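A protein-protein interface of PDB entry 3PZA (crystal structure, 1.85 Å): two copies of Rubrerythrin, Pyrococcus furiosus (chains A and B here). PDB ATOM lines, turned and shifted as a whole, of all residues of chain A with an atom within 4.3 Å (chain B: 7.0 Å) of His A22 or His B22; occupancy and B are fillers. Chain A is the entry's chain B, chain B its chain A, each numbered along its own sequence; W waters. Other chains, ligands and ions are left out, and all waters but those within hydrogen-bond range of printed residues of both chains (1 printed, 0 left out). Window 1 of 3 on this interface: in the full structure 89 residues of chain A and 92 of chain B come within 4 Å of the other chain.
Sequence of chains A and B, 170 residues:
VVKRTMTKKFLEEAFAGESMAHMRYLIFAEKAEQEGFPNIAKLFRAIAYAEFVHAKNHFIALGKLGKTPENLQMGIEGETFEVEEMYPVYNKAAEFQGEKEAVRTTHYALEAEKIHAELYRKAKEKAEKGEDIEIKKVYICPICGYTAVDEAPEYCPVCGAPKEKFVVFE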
ATOM      1  N   GLU A  18       1.128  26.471   7.789  1.00  0.00           N
ATOM      2  CA  GLU A  18       1.482  25.121   7.504  1.00  0.00           C
ATOM      3  C   GLU A  18       1.899  24.968   6.019  1.00  0.00           C
ATOM      4  O   GLU A  18       2.778  24.226   5.722  1.00  0.00           O
ATOM      5  CB  GLU A  18       0.229  24.222   7.653  1.00  0.00           C
ATOM      6  CG  GLU A  18      -0.170  24.090   9.204  1.00  0.00           C
ATOM      7  CD  GLU A  18       0.812  23.180   9.953  1.00  0.00           C
ATOM      8  OE1 GLU A  18       1.716  22.447   9.414  1.00  0.00           O
ATOM      9  OE2 GLU A  18       0.871  23.138  11.200  1.00  0.00           O
ATOM     10  N   SER A  19       1.221  25.685   5.109  1.00  0.00           N
ATOM     11  CA  SER A  19       1.623  25.561   3.660  1.00  0.00           C
ATOM     12  C   SER A  19       3.045  26.043   3.469  1.00  0.00           C
ATOM     13  O   SER A  19       3.794  25.522   2.632  1.00  0.00           O
ATOM     14  CB  SER A  19       0.675  26.507   2.867  1.00  0.00           C
ATOM     15  OG  SER A  19      -0.645  25.909   2.881  1.00  0.00           O
ATOM     16  N   MET A  20       3.360  27.188   4.083  1.00  0.00           N
ATOM     17  CA  MET A  20       4.714  27.807   3.959  1.00  0.00           C
ATOM     18  C   MET A  20       5.768  26.939   4.674  1.00  0.00           C
ATOM     19  O   MET A  20       6.851  26.736   4.139  1.00  0.00           O
ATOM     20  CB  MET A  20       4.806  29.224   4.544  1.00  0.00           C
ATOM     21  CG  MET A  20       4.095  30.203   3.592  1.00  0.00           C
ATOM     22  SD  MET A  20       4.272  31.907   4.070  1.00  0.00           S
ATOM     23  CE  MET A  20       3.031  31.996   5.226  1.00  0.00           C
ATOM     24  N   ALA A  21       5.392  26.328   5.810  1.00  0.00           N
ATOM     25  CA  ALA A  21       6.363  25.347   6.480  1.00  0.00           C
ATOM     26  C   ALA A  21       6.628  24.136   5.565  1.00  0.00           C
ATOM     27  O   ALA A  21       7.780  23.725   5.298  1.00  0.00           O
ATOM     28  CB  ALA A  21       5.796  24.918   7.876  1.00  0.00           C
ATOM     29  N   HIS A  22       5.561  23.542   5.036  1.00  0.00           N
ATOM     30  CA  HIS A  22       5.690  22.465   4.032  1.00  0.00           C
ATOM     31  C   HIS A  22       6.576  22.864   2.904  1.00  0.00           C
ATOM     32  O   HIS A  22       7.460  22.132   2.518  1.00  0.00           O
ATOM     33  CB  HIS A  22       4.271  22.106   3.516  1.00  0.00           C
ATOM     34  CG  HIS A  22       4.275  21.159   2.352  1.00  0.00           C
ATOM     35  ND1 HIS A  22       4.191  19.788   2.523  1.00  0.00           N
ATOM     36  CD2 HIS A  22       4.286  21.371   1.001  1.00  0.00           C
ATOM     37  CE1 HIS A  22       4.196  19.184   1.326  1.00  0.00           C
ATOM     38  NE2 HIS A  22       4.261  20.124   0.392  1.00  0.00           N
ATOM     39  N   MET A  23       6.356  24.051   2.342  1.00  0.00           N
ATOM     40  CA  MET A  23       7.159  24.457   1.186  1.00  0.00           C
ATOM     41  C   MET A  23       8.652  24.718   1.553  1.00  0.00           C
ATOM     42  O   MET A  23       9.580  24.282   0.860  1.00  0.00           O
ATOM     43  CB  MET A  23       6.540  25.762   0.662  1.00  0.00           C
ATOM     44  CG  MET A  23       7.233  26.276  -0.636  1.00  0.00           C
ATOM     45  SD  MET A  23       7.163  25.136  -2.030  1.00  0.00           S
ATOM     46  CE  MET A  23       5.366  25.195  -2.449  1.00  0.00           C
ATOM     47  N   ARG A  24       8.908  25.399   2.673  1.00  0.00           N
ATOM     48  CA  ARG A  24      10.322  25.595   3.074  1.00  0.00           C
ATOM     49  C   ARG A  24      10.958  24.247   3.233  1.00  0.00           C
ATOM     50  O   ARG A  24      12.140  24.091   2.881  1.00  0.00           O
ATOM     51  CB  ARG A  24      10.368  26.383   4.412  1.00  0.00           C
ATOM     52  CG  ARG A  24      10.078  27.897   4.247  1.00  0.00           C
ATOM     53  CD  ARG A  24      10.380  28.723   5.565  1.00  0.00           C
ATOM     54  NE  ARG A  24       9.631  28.209   6.682  1.00  0.00           N
ATOM     55  CZ  ARG A  24       8.430  28.698   7.027  1.00  0.00           C
ATOM     56  NH1 ARG A  24       7.797  28.179   8.042  1.00  0.00           N
ATOM     57  NH2 ARG A  24       7.907  29.743   6.386  1.00  0.00           N
ATOM     58  N   TYR A  25      10.219  23.281   3.811  1.00  0.00           N
ATOM     59  CA  TYR A  25      10.857  21.936   4.086  1.00  0.00           C
ATOM     60  C   TYR A  25      11.173  21.184   2.803  1.00  0.00           C
ATOM     61  O   TYR A  25      12.190  20.554   2.698  1.00  0.00           O
ATOM     62  CB  TYR A  25       9.981  21.050   4.994  1.00  0.00           C
ATOM     63  CG  TYR A  25       9.866  21.708   6.408  1.00  0.00           C
ATOM     64  CD1 TYR A  25       8.838  21.326   7.263  1.00  0.00           C
ATOM     65  CD2 TYR A  25      10.756  22.739   6.832  1.00  0.00           C
ATOM     66  CE1 TYR A  25       8.702  21.959   8.557  1.00  0.00           C
ATOM     67  CE2 TYR A  25      10.611  23.404   8.118  1.00  0.00           C
ATOM     68  CZ  TYR A  25       9.620  22.966   8.958  1.00  0.00           C
ATOM     69  OH  TYR A  25       9.462  23.601  10.164  1.00  0.00           O
ATOM     70  N   LEU A  26      10.322  21.338   1.790  1.00  0.00           N
ATOM     71  CA  LEU A  26      10.679  20.775   0.482  1.00  0.00           C
ATOM     72  C   LEU A  26      11.913  21.433  -0.151  1.00  0.00           C
ATOM     73  O   LEU A  26      12.719  20.714  -0.803  1.00  0.00           O
ATOM     74  CB  LEU A  26       9.442  20.873  -0.472  1.00  0.00           C
ATOM     75  CG  LEU A  26       8.262  19.935  -0.158  1.00  0.00           C
ATOM     76  CD1 LEU A  26       7.186  20.104  -1.374  1.00  0.00           C
ATOM     77  CD2 LEU A  26       8.702  18.435  -0.016  1.00  0.00           C
ATOM     78  N   ALA A  48       7.696  17.611   6.023  1.00  0.00           N
ATOM     79  CA  ALA A  48       6.834  18.306   5.011  1.00  0.00           C
ATOM     80  C   ALA A  48       5.493  17.597   4.846  1.00  0.00           C
ATOM     81  O   ALA A  48       4.460  18.244   4.766  1.00  0.00           O
ATOM     82  CB  ALA A  48       7.584  18.352   3.649  1.00  0.00           C
ATOM     83  N   GLU A  51       3.215  18.321   7.646  1.00  0.00           N
ATOM     84  CA  GLU A  51       2.580  19.686   7.635  1.00  0.00           C
ATOM     85  C   GLU A  51       1.487  19.736   6.547  1.00  0.00           C
ATOM     86  O   GLU A  51       0.541  20.510   6.672  1.00  0.00           O
ATOM     87  CB  GLU A  51       3.642  20.735   7.288  1.00  0.00           C
ATOM     88  CG  GLU A  51       4.950  20.726   8.055  1.00  0.00           C
ATOM     89  CD  GLU A  51       4.795  20.768   9.596  1.00  0.00           C
ATOM     90  OE1 GLU A  51       3.651  20.807  10.135  1.00  0.00           O
ATOM     91  OE2 GLU A  51       5.899  21.000  10.254  1.00  0.00           O
ATOM     92  N   PHE A  52       1.631  18.918   5.496  1.00  0.00           N
ATOM     93  CA  PHE A  52       0.447  18.682   4.597  1.00  0.00           C
ATOM     94  C   PHE A  52      -0.804  18.125   5.361  1.00  0.00           C
ATOM     95  O   PHE A  52      -1.960  18.574   5.136  1.00  0.00           O
ATOM     96  CB  PHE A  52       0.896  17.836   3.370  1.00  0.00           C
ATOM     97  CG  PHE A  52      -0.246  17.030   2.729  1.00  0.00           C
ATOM     98  CD1 PHE A  52      -0.986  17.608   1.686  1.00  0.00           C
ATOM     99  CD2 PHE A  52      -0.630  15.751   3.196  1.00  0.00           C
ATOM    100  CE1 PHE A  52      -2.076  16.920   1.049  1.00  0.00           C
ATOM    101  CE2 PHE A  52      -1.765  15.073   2.622  1.00  0.00           C
ATOM    102  CZ  PHE A  52      -2.508  15.677   1.531  1.00  0.00           C
ATOM    103  N   ALA B  16       3.804  33.132  -0.033  1.00  0.00           N
ATOM    104  CA  ALA B  16       2.657  32.581   0.681  1.00  0.00           C
ATOM    105  C   ALA B  16       1.581  32.041  -0.302  1.00  0.00           C
ATOM    106  O   ALA B  16       1.011  30.988  -0.134  1.00  0.00           O
ATOM    107  CB  ALA B  16       2.048  33.621   1.585  1.00  0.00           C
ATOM    108  N   GLY B  17       1.352  32.799  -1.380  1.00  0.00           N
ATOM    109  CA  GLY B  17       0.284  32.428  -2.387  1.00  0.00           C
ATOM    110  C   GLY B  17       0.659  31.160  -3.124  1.00  0.00           C
ATOM    111  O   GLY B  17      -0.215  30.309  -3.297  1.00  0.00           O
ATOM    112  N   GLU B  18       1.955  31.040  -3.537  1.00  0.00           N
ATOM    113  CA  GLU B  18       2.396  29.812  -4.218  1.00  0.00           C
ATOM    114  C   GLU B  18       2.402  28.613  -3.270  1.00  0.00           C
ATOM    115  O   GLU B  18       1.979  27.527  -3.650  1.00  0.00           O
ATOM    116  CB  GLU B  18       3.862  29.976  -4.653  1.00  0.00           C
ATOM    117  CG  GLU B  18       4.001  31.035  -5.840  1.00  0.00           C
ATOM    118  CD  GLU B  18       3.435  30.525  -7.191  1.00  0.00           C
ATOM    119  OE1 GLU B  18       3.140  31.232  -8.142  1.00  0.00           O
ATOM    120  OE2 GLU B  18       3.142  29.342  -7.402  1.00  0.00           O
ATOM    121  N   SER B  19       2.840  28.851  -2.011  1.00  0.00           N
ATOM    122  CA  SER B  19       2.797  27.755  -1.024  1.00  0.00           C
ATOM    123  C   SER B  19       1.354  27.249  -0.871  1.00  0.00           C
ATOM    124  O   SER B  19       1.105  25.965  -0.794  1.00  0.00           O
ATOM    125  CB  SER B  19       3.299  28.284   0.309  1.00  0.00           C
ATOM    126  OG  SER B  19       4.728  28.561   0.202  1.00  0.00           O
ATOM    127  N   MET B  20       0.403  28.174  -0.752  1.00  0.00           N
ATOM    128  CA  MET B  20      -1.004  27.745  -0.507  1.00  0.00           C
ATOM    129  C   MET B  20      -1.612  27.088  -1.755  1.00  0.00           C
ATOM    130  O   MET B  20      -2.329  26.114  -1.629  1.00  0.00           O
ATOM    131  CB  MET B  20      -1.949  28.909  -0.077  1.00  0.00           C
ATOM    132  CG  MET B  20      -1.569  29.282   1.417  1.00  0.00           C
ATOM    133  SD  MET B  20      -2.736  30.541   2.009  1.00  0.00           S
ATOM    134  CE  MET B  20      -2.091  31.912   1.147  1.00  0.00           C
ATOM    135  N   ALA B  21      -1.208  27.553  -2.950  1.00  0.00           N
ATOM    136  CA  ALA B  21      -1.733  26.916  -4.180  1.00  0.00           C
ATOM    137  C   ALA B  21      -1.174  25.473  -4.281  1.00  0.00           C
ATOM    138  O   ALA B  21      -1.890  24.535  -4.573  1.00  0.00           O
ATOM    139  CB  ALA B  21      -1.271  27.767  -5.438  1.00  0.00           C
ATOM    140  N   HIS B  22       0.114  25.308  -4.048  1.00  0.00           N
ATOM    141  CA  HIS B  22       0.798  23.955  -4.005  1.00  0.00           C
ATOM    142  C   HIS B  22       0.023  23.079  -3.061  1.00  0.00           C
ATOM    143  O   HIS B  22      -0.333  21.950  -3.403  1.00  0.00           O
ATOM    144  CB  HIS B  22       2.224  24.156  -3.576  1.00  0.00           C
ATOM    145  CG  HIS B  22       2.920  22.881  -3.243  1.00  0.00           C
ATOM    146  ND1 HIS B  22       3.633  22.204  -4.186  1.00  0.00           N
ATOM    147  CD2 HIS B  22       3.069  22.194  -2.071  1.00  0.00           C
ATOM    148  CE1 HIS B  22       4.161  21.098  -3.629  1.00  0.00           C
ATOM    149  NE2 HIS B  22       3.858  21.092  -2.333  1.00  0.00           N
ATOM    150  N   MET B  23      -0.259  23.613  -1.865  1.00  0.00           N
ATOM    151  CA  MET B  23      -0.912  22.771  -0.814  1.00  0.00           C
ATOM    152  C   MET B  23      -2.340  22.441  -1.273  1.00  0.00           C
ATOM    153  O   MET B  23      -2.783  21.280  -1.202  1.00  0.00           O
ATOM    154  CB  MET B  23      -0.929  23.538   0.527  1.00  0.00           C
ATOM    155  CG  MET B  23      -1.586  22.741   1.651  1.00  0.00           C
ATOM    156  SD  MET B  23      -0.628  21.223   2.001  1.00  0.00           S
ATOM    157  CE  MET B  23       0.887  21.893   2.786  1.00  0.00           C
ATOM    158  N   ARG B  24      -3.077  23.432  -1.777  1.00  0.00           N
ATOM    159  CA  ARG B  24      -4.407  23.100  -2.235  1.00  0.00           C
ATOM    160  C   ARG B  24      -4.378  21.985  -3.299  1.00  0.00           C
ATOM    161  O   ARG B  24      -5.215  21.075  -3.352  1.00  0.00           O
ATOM    162  CB  ARG B  24      -5.060  24.381  -2.827  1.00  0.00           C
ATOM    163  CG  ARG B  24      -5.629  25.301  -1.703  1.00  0.00           C
ATOM    164  CD  ARG B  24      -6.570  26.478  -2.193  1.00  0.00           C
ATOM    165  NE  ARG B  24      -5.883  27.233  -3.181  1.00  0.00           N
ATOM    166  CZ  ARG B  24      -5.195  28.352  -2.940  1.00  0.00           C
ATOM    167  NH1 ARG B  24      -4.573  28.924  -3.952  1.00  0.00           N
ATOM    168  NH2 ARG B  24      -5.194  28.913  -1.736  1.00  0.00           N
ATOM    169  N   TYR B  25      -3.459  22.114  -4.240  1.00  0.00           N
ATOM    170  CA  TYR B  25      -3.396  21.173  -5.334  1.00  0.00           C
ATOM    171  C   TYR B  25      -3.057  19.773  -4.838  1.00  0.00           C
ATOM    172  O   TYR B  25      -3.573  18.817  -5.385  1.00  0.00           O
ATOM    173  CB  TYR B  25      -2.401  21.598  -6.460  1.00  0.00           C
ATOM    174  CG  TYR B  25      -2.852  22.901  -7.120  1.00  0.00           C
ATOM    175  CD1 TYR B  25      -1.943  23.728  -7.813  1.00  0.00           C
ATOM    176  CD2 TYR B  25      -4.214  23.356  -6.985  1.00  0.00           C
ATOM    177  CE1 TYR B  25      -2.363  25.028  -8.324  1.00  0.00           C
ATOM    178  CE2 TYR B  25      -4.615  24.615  -7.535  1.00  0.00           C
ATOM    179  CZ  TYR B  25      -3.682  25.404  -8.214  1.00  0.00           C
ATOM    180  OH  TYR B  25      -4.027  26.637  -8.775  1.00  0.00           O
ATOM    181  N   LEU B  26      -2.198  19.649  -3.827  1.00  0.00           N
ATOM    182  CA  LEU B  26      -1.928  18.286  -3.269  1.00  0.00           C
ATOM    183  C   LEU B  26      -3.223  17.736  -2.605  1.00  0.00           C
ATOM    184  O   LEU B  26      -3.502  16.512  -2.713  1.00  0.00           O
ATOM    185  CB  LEU B  26      -0.792  18.309  -2.254  1.00  0.00           C
ATOM    186  CG  LEU B  26       0.588  18.612  -2.823  1.00  0.00           C
ATOM    187  CD1 LEU B  26       1.633  18.541  -1.625  1.00  0.00           C
ATOM    188  CD2 LEU B  26       1.044  17.679  -3.950  1.00  0.00           C
ATOM    189  N   ILE B  27      -3.949  18.579  -1.911  1.00  0.00           N
ATOM    190  CA  ILE B  27      -5.152  18.137  -1.210  1.00  0.00           C
ATOM    191  C   ILE B  27      -6.148  17.696  -2.356  1.00  0.00           C
ATOM    192  O   ILE B  27      -6.875  16.662  -2.250  1.00  0.00           O
ATOM    193  CB  ILE B  27      -5.725  19.240  -0.325  1.00  0.00           C
ATOM    194  CG1 ILE B  27      -4.775  19.539   0.853  1.00  0.00           C
ATOM    195  CG2 ILE B  27      -7.243  18.964   0.212  1.00  0.00           C
ATOM    196  CD1 ILE B  27      -5.183  20.841   1.551  1.00  0.00           C
ATOM    197  N   PHE B  28      -6.257  18.554  -3.380  1.00  0.00           N
ATOM    198  CA  PHE B  28      -7.205  18.270  -4.544  1.00  0.00           C
ATOM    199  C   PHE B  28      -6.793  16.995  -5.326  1.00  0.00           C
ATOM    200  O   PHE B  28      -7.697  16.242  -5.778  1.00  0.00           O
ATOM    201  CB  PHE B  28      -7.272  19.439  -5.508  1.00  0.00           C
ATOM    202  CG  PHE B  28      -7.869  20.694  -4.959  1.00  0.00           C
ATOM    203  CD1 PHE B  28      -7.627  21.894  -5.625  1.00  0.00           C
ATOM    204  CD2 PHE B  28      -8.634  20.693  -3.748  1.00  0.00           C
ATOM    205  CE1 PHE B  28      -8.213  23.090  -5.120  1.00  0.00           C
ATOM    206  CE2 PHE B  28      -9.189  21.852  -3.269  1.00  0.00           C
ATOM    207  CZ  PHE B  28      -8.987  23.046  -3.952  1.00  0.00           C
ATOM    208  N   PHE B  44      -3.112  17.755 -11.130  1.00  0.00           N
ATOM    209  CA  PHE B  44      -2.934  18.554  -9.833  1.00  0.00           C
ATOM    210  C   PHE B  44      -1.560  18.334  -9.270  1.00  0.00           C
ATOM    211  O   PHE B  44      -0.917  19.297  -8.837  1.00  0.00           O
ATOM    212  CB  PHE B  44      -3.968  18.146  -8.761  1.00  0.00           C
ATOM    213  CG  PHE B  44      -5.308  18.827  -8.881  1.00  0.00           C
ATOM    214  CD1 PHE B  44      -5.409  20.233  -8.942  1.00  0.00           C
ATOM    215  CD2 PHE B  44      -6.480  18.060  -8.961  1.00  0.00           C
ATOM    216  CE1 PHE B  44      -6.718  20.868  -9.019  1.00  0.00           C
ATOM    217  CE2 PHE B  44      -7.775  18.682  -9.016  1.00  0.00           C
ATOM    218  CZ  PHE B  44      -7.879  20.075  -9.072  1.00  0.00           C
ATOM    219  N   ARG B  45      -1.074  17.092  -9.245  1.00  0.00           N
ATOM    220  CA  ARG B  45       0.288  16.879  -8.706  1.00  0.00           C
ATOM    221  C   ARG B  45       1.408  17.575  -9.498  1.00  0.00           C
ATOM    222  O   ARG B  45       2.383  18.105  -8.934  1.00  0.00           O
ATOM    223  CB  ARG B  45       0.575  15.353  -8.659  1.00  0.00           C
ATOM    224  CG  ARG B  45      -0.201  14.674  -7.519  1.00  0.00           C
ATOM    225  CD  ARG B  45       0.262  13.210  -7.412  1.00  0.00           C
ATOM    226  NE  ARG B  45      -0.828  12.435  -6.862  1.00  0.00           N
ATOM    227  CZ  ARG B  45      -1.536  11.565  -7.589  1.00  0.00           C
ATOM    228  NH1 ARG B  45      -1.223  11.327  -8.895  1.00  0.00           N
ATOM    229  NH2 ARG B  45      -2.518  10.908  -6.987  1.00  0.00           N
ATOM    230  N   ILE B  47       1.084  20.196 -11.463  1.00  0.00           N
ATOM    231  CA  ILE B  47       0.989  21.652 -11.343  1.00  0.00           C
ATOM    232  C   ILE B  47       1.426  22.046  -9.894  1.00  0.00           C
ATOM    233  O   ILE B  47       2.069  23.063  -9.670  1.00  0.00           O
ATOM    234  CB  ILE B  47      -0.441  22.127 -11.702  1.00  0.00           C
ATOM    235  CG1 ILE B  47      -0.602  22.027 -13.248  1.00  0.00           C
ATOM    236  CG2 ILE B  47      -0.620  23.629 -11.289  1.00  0.00           C
ATOM    237  CD1 ILE B  47      -2.063  22.478 -13.648  1.00  0.00           C
ATOM    238  N   ALA B  48       1.122  21.182  -8.915  1.00  0.00           N
ATOM    239  CA  ALA B  48       1.685  21.536  -7.545  1.00  0.00           C
ATOM    240  C   ALA B  48       3.219  21.606  -7.627  1.00  0.00           C
ATOM    241  O   ALA B  48       3.774  22.412  -6.904  1.00  0.00           O
ATOM    242  CB  ALA B  48       1.302  20.357  -6.514  1.00  0.00           C
ATOM    243  N   TYR B  49       3.896  20.753  -8.424  1.00  0.00           N
ATOM    244  CA  TYR B  49       5.326  20.841  -8.509  1.00  0.00           C
ATOM    245  C   TYR B  49       5.758  22.178  -9.157  1.00  0.00           C
ATOM    246  O   TYR B  49       6.745  22.774  -8.763  1.00  0.00           O
ATOM    247  CB  TYR B  49       5.956  19.632  -9.248  1.00  0.00           C
ATOM    248  CG  TYR B  49       7.481  19.782  -9.445  1.00  0.00           C
ATOM    249  CD1 TYR B  49       8.412  19.687  -8.369  1.00  0.00           C
ATOM    250  CD2 TYR B  49       7.986  20.058 -10.695  1.00  0.00           C
ATOM    251  CE1 TYR B  49       9.811  19.867  -8.577  1.00  0.00           C
ATOM    252  CE2 TYR B  49       9.370  20.247 -10.890  1.00  0.00           C
ATOM    253  CZ  TYR B  49      10.236  20.132  -9.864  1.00  0.00           C
ATOM    254  OH  TYR B  49      11.562  20.343 -10.134  1.00  0.00           O
ATOM    255  N   ALA B  50       5.045  22.618 -10.184  1.00  0.00           N
ATOM    256  CA  ALA B  50       5.293  23.934 -10.800  1.00  0.00           C
ATOM    257  C   ALA B  50       5.194  24.989  -9.777  1.00  0.00           C
ATOM    258  O   ALA B  50       5.974  25.901  -9.805  1.00  0.00           O
ATOM    259  CB  ALA B  50       4.221  24.184 -11.954  1.00  0.00           C
ATOM    260  N   GLU B  51       4.237  24.907  -8.865  1.00  0.00           N
ATOM    261  CA  GLU B  51       4.165  25.974  -7.848  1.00  0.00           C
ATOM    262  C   GLU B  51       5.276  25.901  -6.829  1.00  0.00           C
ATOM    263  O   GLU B  51       5.610  26.920  -6.266  1.00  0.00           O
ATOM    264  CB  GLU B  51       2.838  25.909  -7.059  1.00  0.00           C
ATOM    265  CG  GLU B  51       1.513  25.738  -7.905  1.00  0.00           C
ATOM    266  CD  GLU B  51       1.312  26.837  -9.036  1.00  0.00           C
ATOM    267  OE1 GLU B  51       0.208  26.816  -9.638  1.00  0.00           O
ATOM    268  OE2 GLU B  51       2.229  27.723  -9.261  1.00  0.00           O
ATOM    269  N   PHE B  52       5.745  24.691  -6.539  1.00  0.00           N
ATOM    270  CA  PHE B  52       7.026  24.536  -5.767  1.00  0.00           C
ATOM    271  C   PHE B  52       8.176  25.300  -6.459  1.00  0.00           C
ATOM    272  O   PHE B  52       8.954  25.985  -5.819  1.00  0.00           O
ATOM    273  CB  PHE B  52       7.385  23.055  -5.601  1.00  0.00           C
ATOM    274  CG  PHE B  52       8.868  22.812  -5.233  1.00  0.00           C
ATOM    275  CD1 PHE B  52       9.278  22.910  -3.883  1.00  0.00           C
ATOM    276  CD2 PHE B  52       9.804  22.481  -6.248  1.00  0.00           C
ATOM    277  CE1 PHE B  52      10.597  22.700  -3.580  1.00  0.00           C
ATOM    278  CE2 PHE B  52      11.103  22.282  -5.961  1.00  0.00           C
ATOM    279  CZ  PHE B  52      11.520  22.407  -4.626  1.00  0.00           C
ATOM    280  N   VAL B  53       8.292  25.163  -7.793  1.00  0.00           N
ATOM    281  CA  VAL B  53       9.295  25.878  -8.467  1.00  0.00           C
ATOM    282  C   VAL B  53       9.129  27.404  -8.305  1.00  0.00           C
ATOM    283  O   VAL B  53      10.136  28.126  -8.051  1.00  0.00           O
ATOM    284  CB  VAL B  53       9.326  25.450  -9.974  1.00  0.00           C
ATOM    285  CG1 VAL B  53      10.409  26.266 -10.693  1.00  0.00           C
ATOM    286  CG2 VAL B  53       9.704  23.917 -10.088  1.00  0.00           C
ATOM    287  N   ALA B  55       7.538  29.061  -5.961  1.00  0.00           N
ATOM    288  CA  ALA B  55       7.823  29.468  -4.573  1.00  0.00           C
ATOM    289  C   ALA B  55       9.306  29.432  -4.238  1.00  0.00           C
ATOM    290  O   ALA B  55       9.771  30.372  -3.597  1.00  0.00           O
ATOM    291  CB  ALA B  55       7.031  28.504  -3.570  1.00  0.00           C
HETATM  292  O   HOH W   1       2.903  24.308   0.390  1.00  0.00           O
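Among the printed residues, pairs that only touch across the chains: Ser A19 with Met B23 (3.4 Å), Met A23 with Ser B19 (3.4 Å), Met A23 with His B22 (3.5 Å), His A22 with Met B23 (3.5 Å), Met A23 with Phe B52 (3.6 Å), Leu A26 with His B22 (3.6 Å), Ser A19 with Ser B19 (3.6 Å), Phe A52 with Met B23 (3.6 Å), His A22 with Leu B26 (3.7 Å), Met A23 with Ala B55 (3.7 Å), Met A20 with Ala B16 (3.7 Å), Phe A52 with Ile B27 (3.8 Å), Leu A26 with Phe B52 (3.8 Å), Ser A19 with Met B20 (3.8 Å), Phe A52 with Leu B26 (3.8 Å) and Met A20 with Ser B19 (3.8 Å).
Of chain B, only His B22 (2.9 Å), Met B23 (3.5 Å) and Leu B26 (3.7 Å) come within 4 Å of His A22.
Printed residues of chain A within 4 Å of Ala B16: Met A20 (3.7 Å).
Of the printed residues of chain A, His B22 touches His A22, Met A23 and Leu A26.
Of the printed residues of chain A, Met B23 touches Ser A19 (3.4 Å), His A22 (3.5 Å) and Phe A52 (3.6 Å).
Val B53 touches none of the printed residues of chain A.
The nearest printed residue of chain A that does not touch His B22 is Ser A19 (5.8 Å).
The nearest printed residue of chain A that does not touch Phe B52 is Tyr A25 (6.6 Å).
Along chain B the printed residues that touch a printed residue of chain A span positions 16 to 55.
Printed residues of chain A that touch a printed residue of chain B: Ser A19, Met A20, His A22, Met A23, Leu A26 and Phe A52.
Hydrophobic or aromatic side chains of chain A within 4 Å of the printed part of chain B: Met A20, His A22, Met A23, Leu A26 and Phe A52.
Among the printed residues, no Asp or Glu carboxylate lies within 4 Å of a Lys or Arg side-chain nitrogen of the other chain.
A ring nitrogen (ND1) of His B22 is in hydrogen-bond range of the backbone carbonyl oxygen of Ala B48 (2.7 Å).
A ring nitrogen (ND1) of His A22 sits at hydrogen-bond distance from the backbone carbonyl oxygen (O) of Ala A48, 2.7 Å away.
A ring nitrogen (NE2) of His B22 is in hydrogen-bond range of a ring nitrogen (NE2) of His A22 (2.9 Å).
Water W1 bridges O of Ser A19 (2.7 Å) and O of Ser B19 (2.7 Å).
Ser A19 touches Met B20, and with the chains exchanged Met A20 touches Ser B19.
His B22 touches its own counterpart, His A22.
His A22 touches Met B23, and with the chains exchanged Met A23 touches His B22.
Met A23 touches Phe B52, and with the chains exchanged Phe A52 touches Met B23.
Of the 17 pairs that touch across the chains among the printed residues, 14 have their exchanged pair printed and touching as well.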
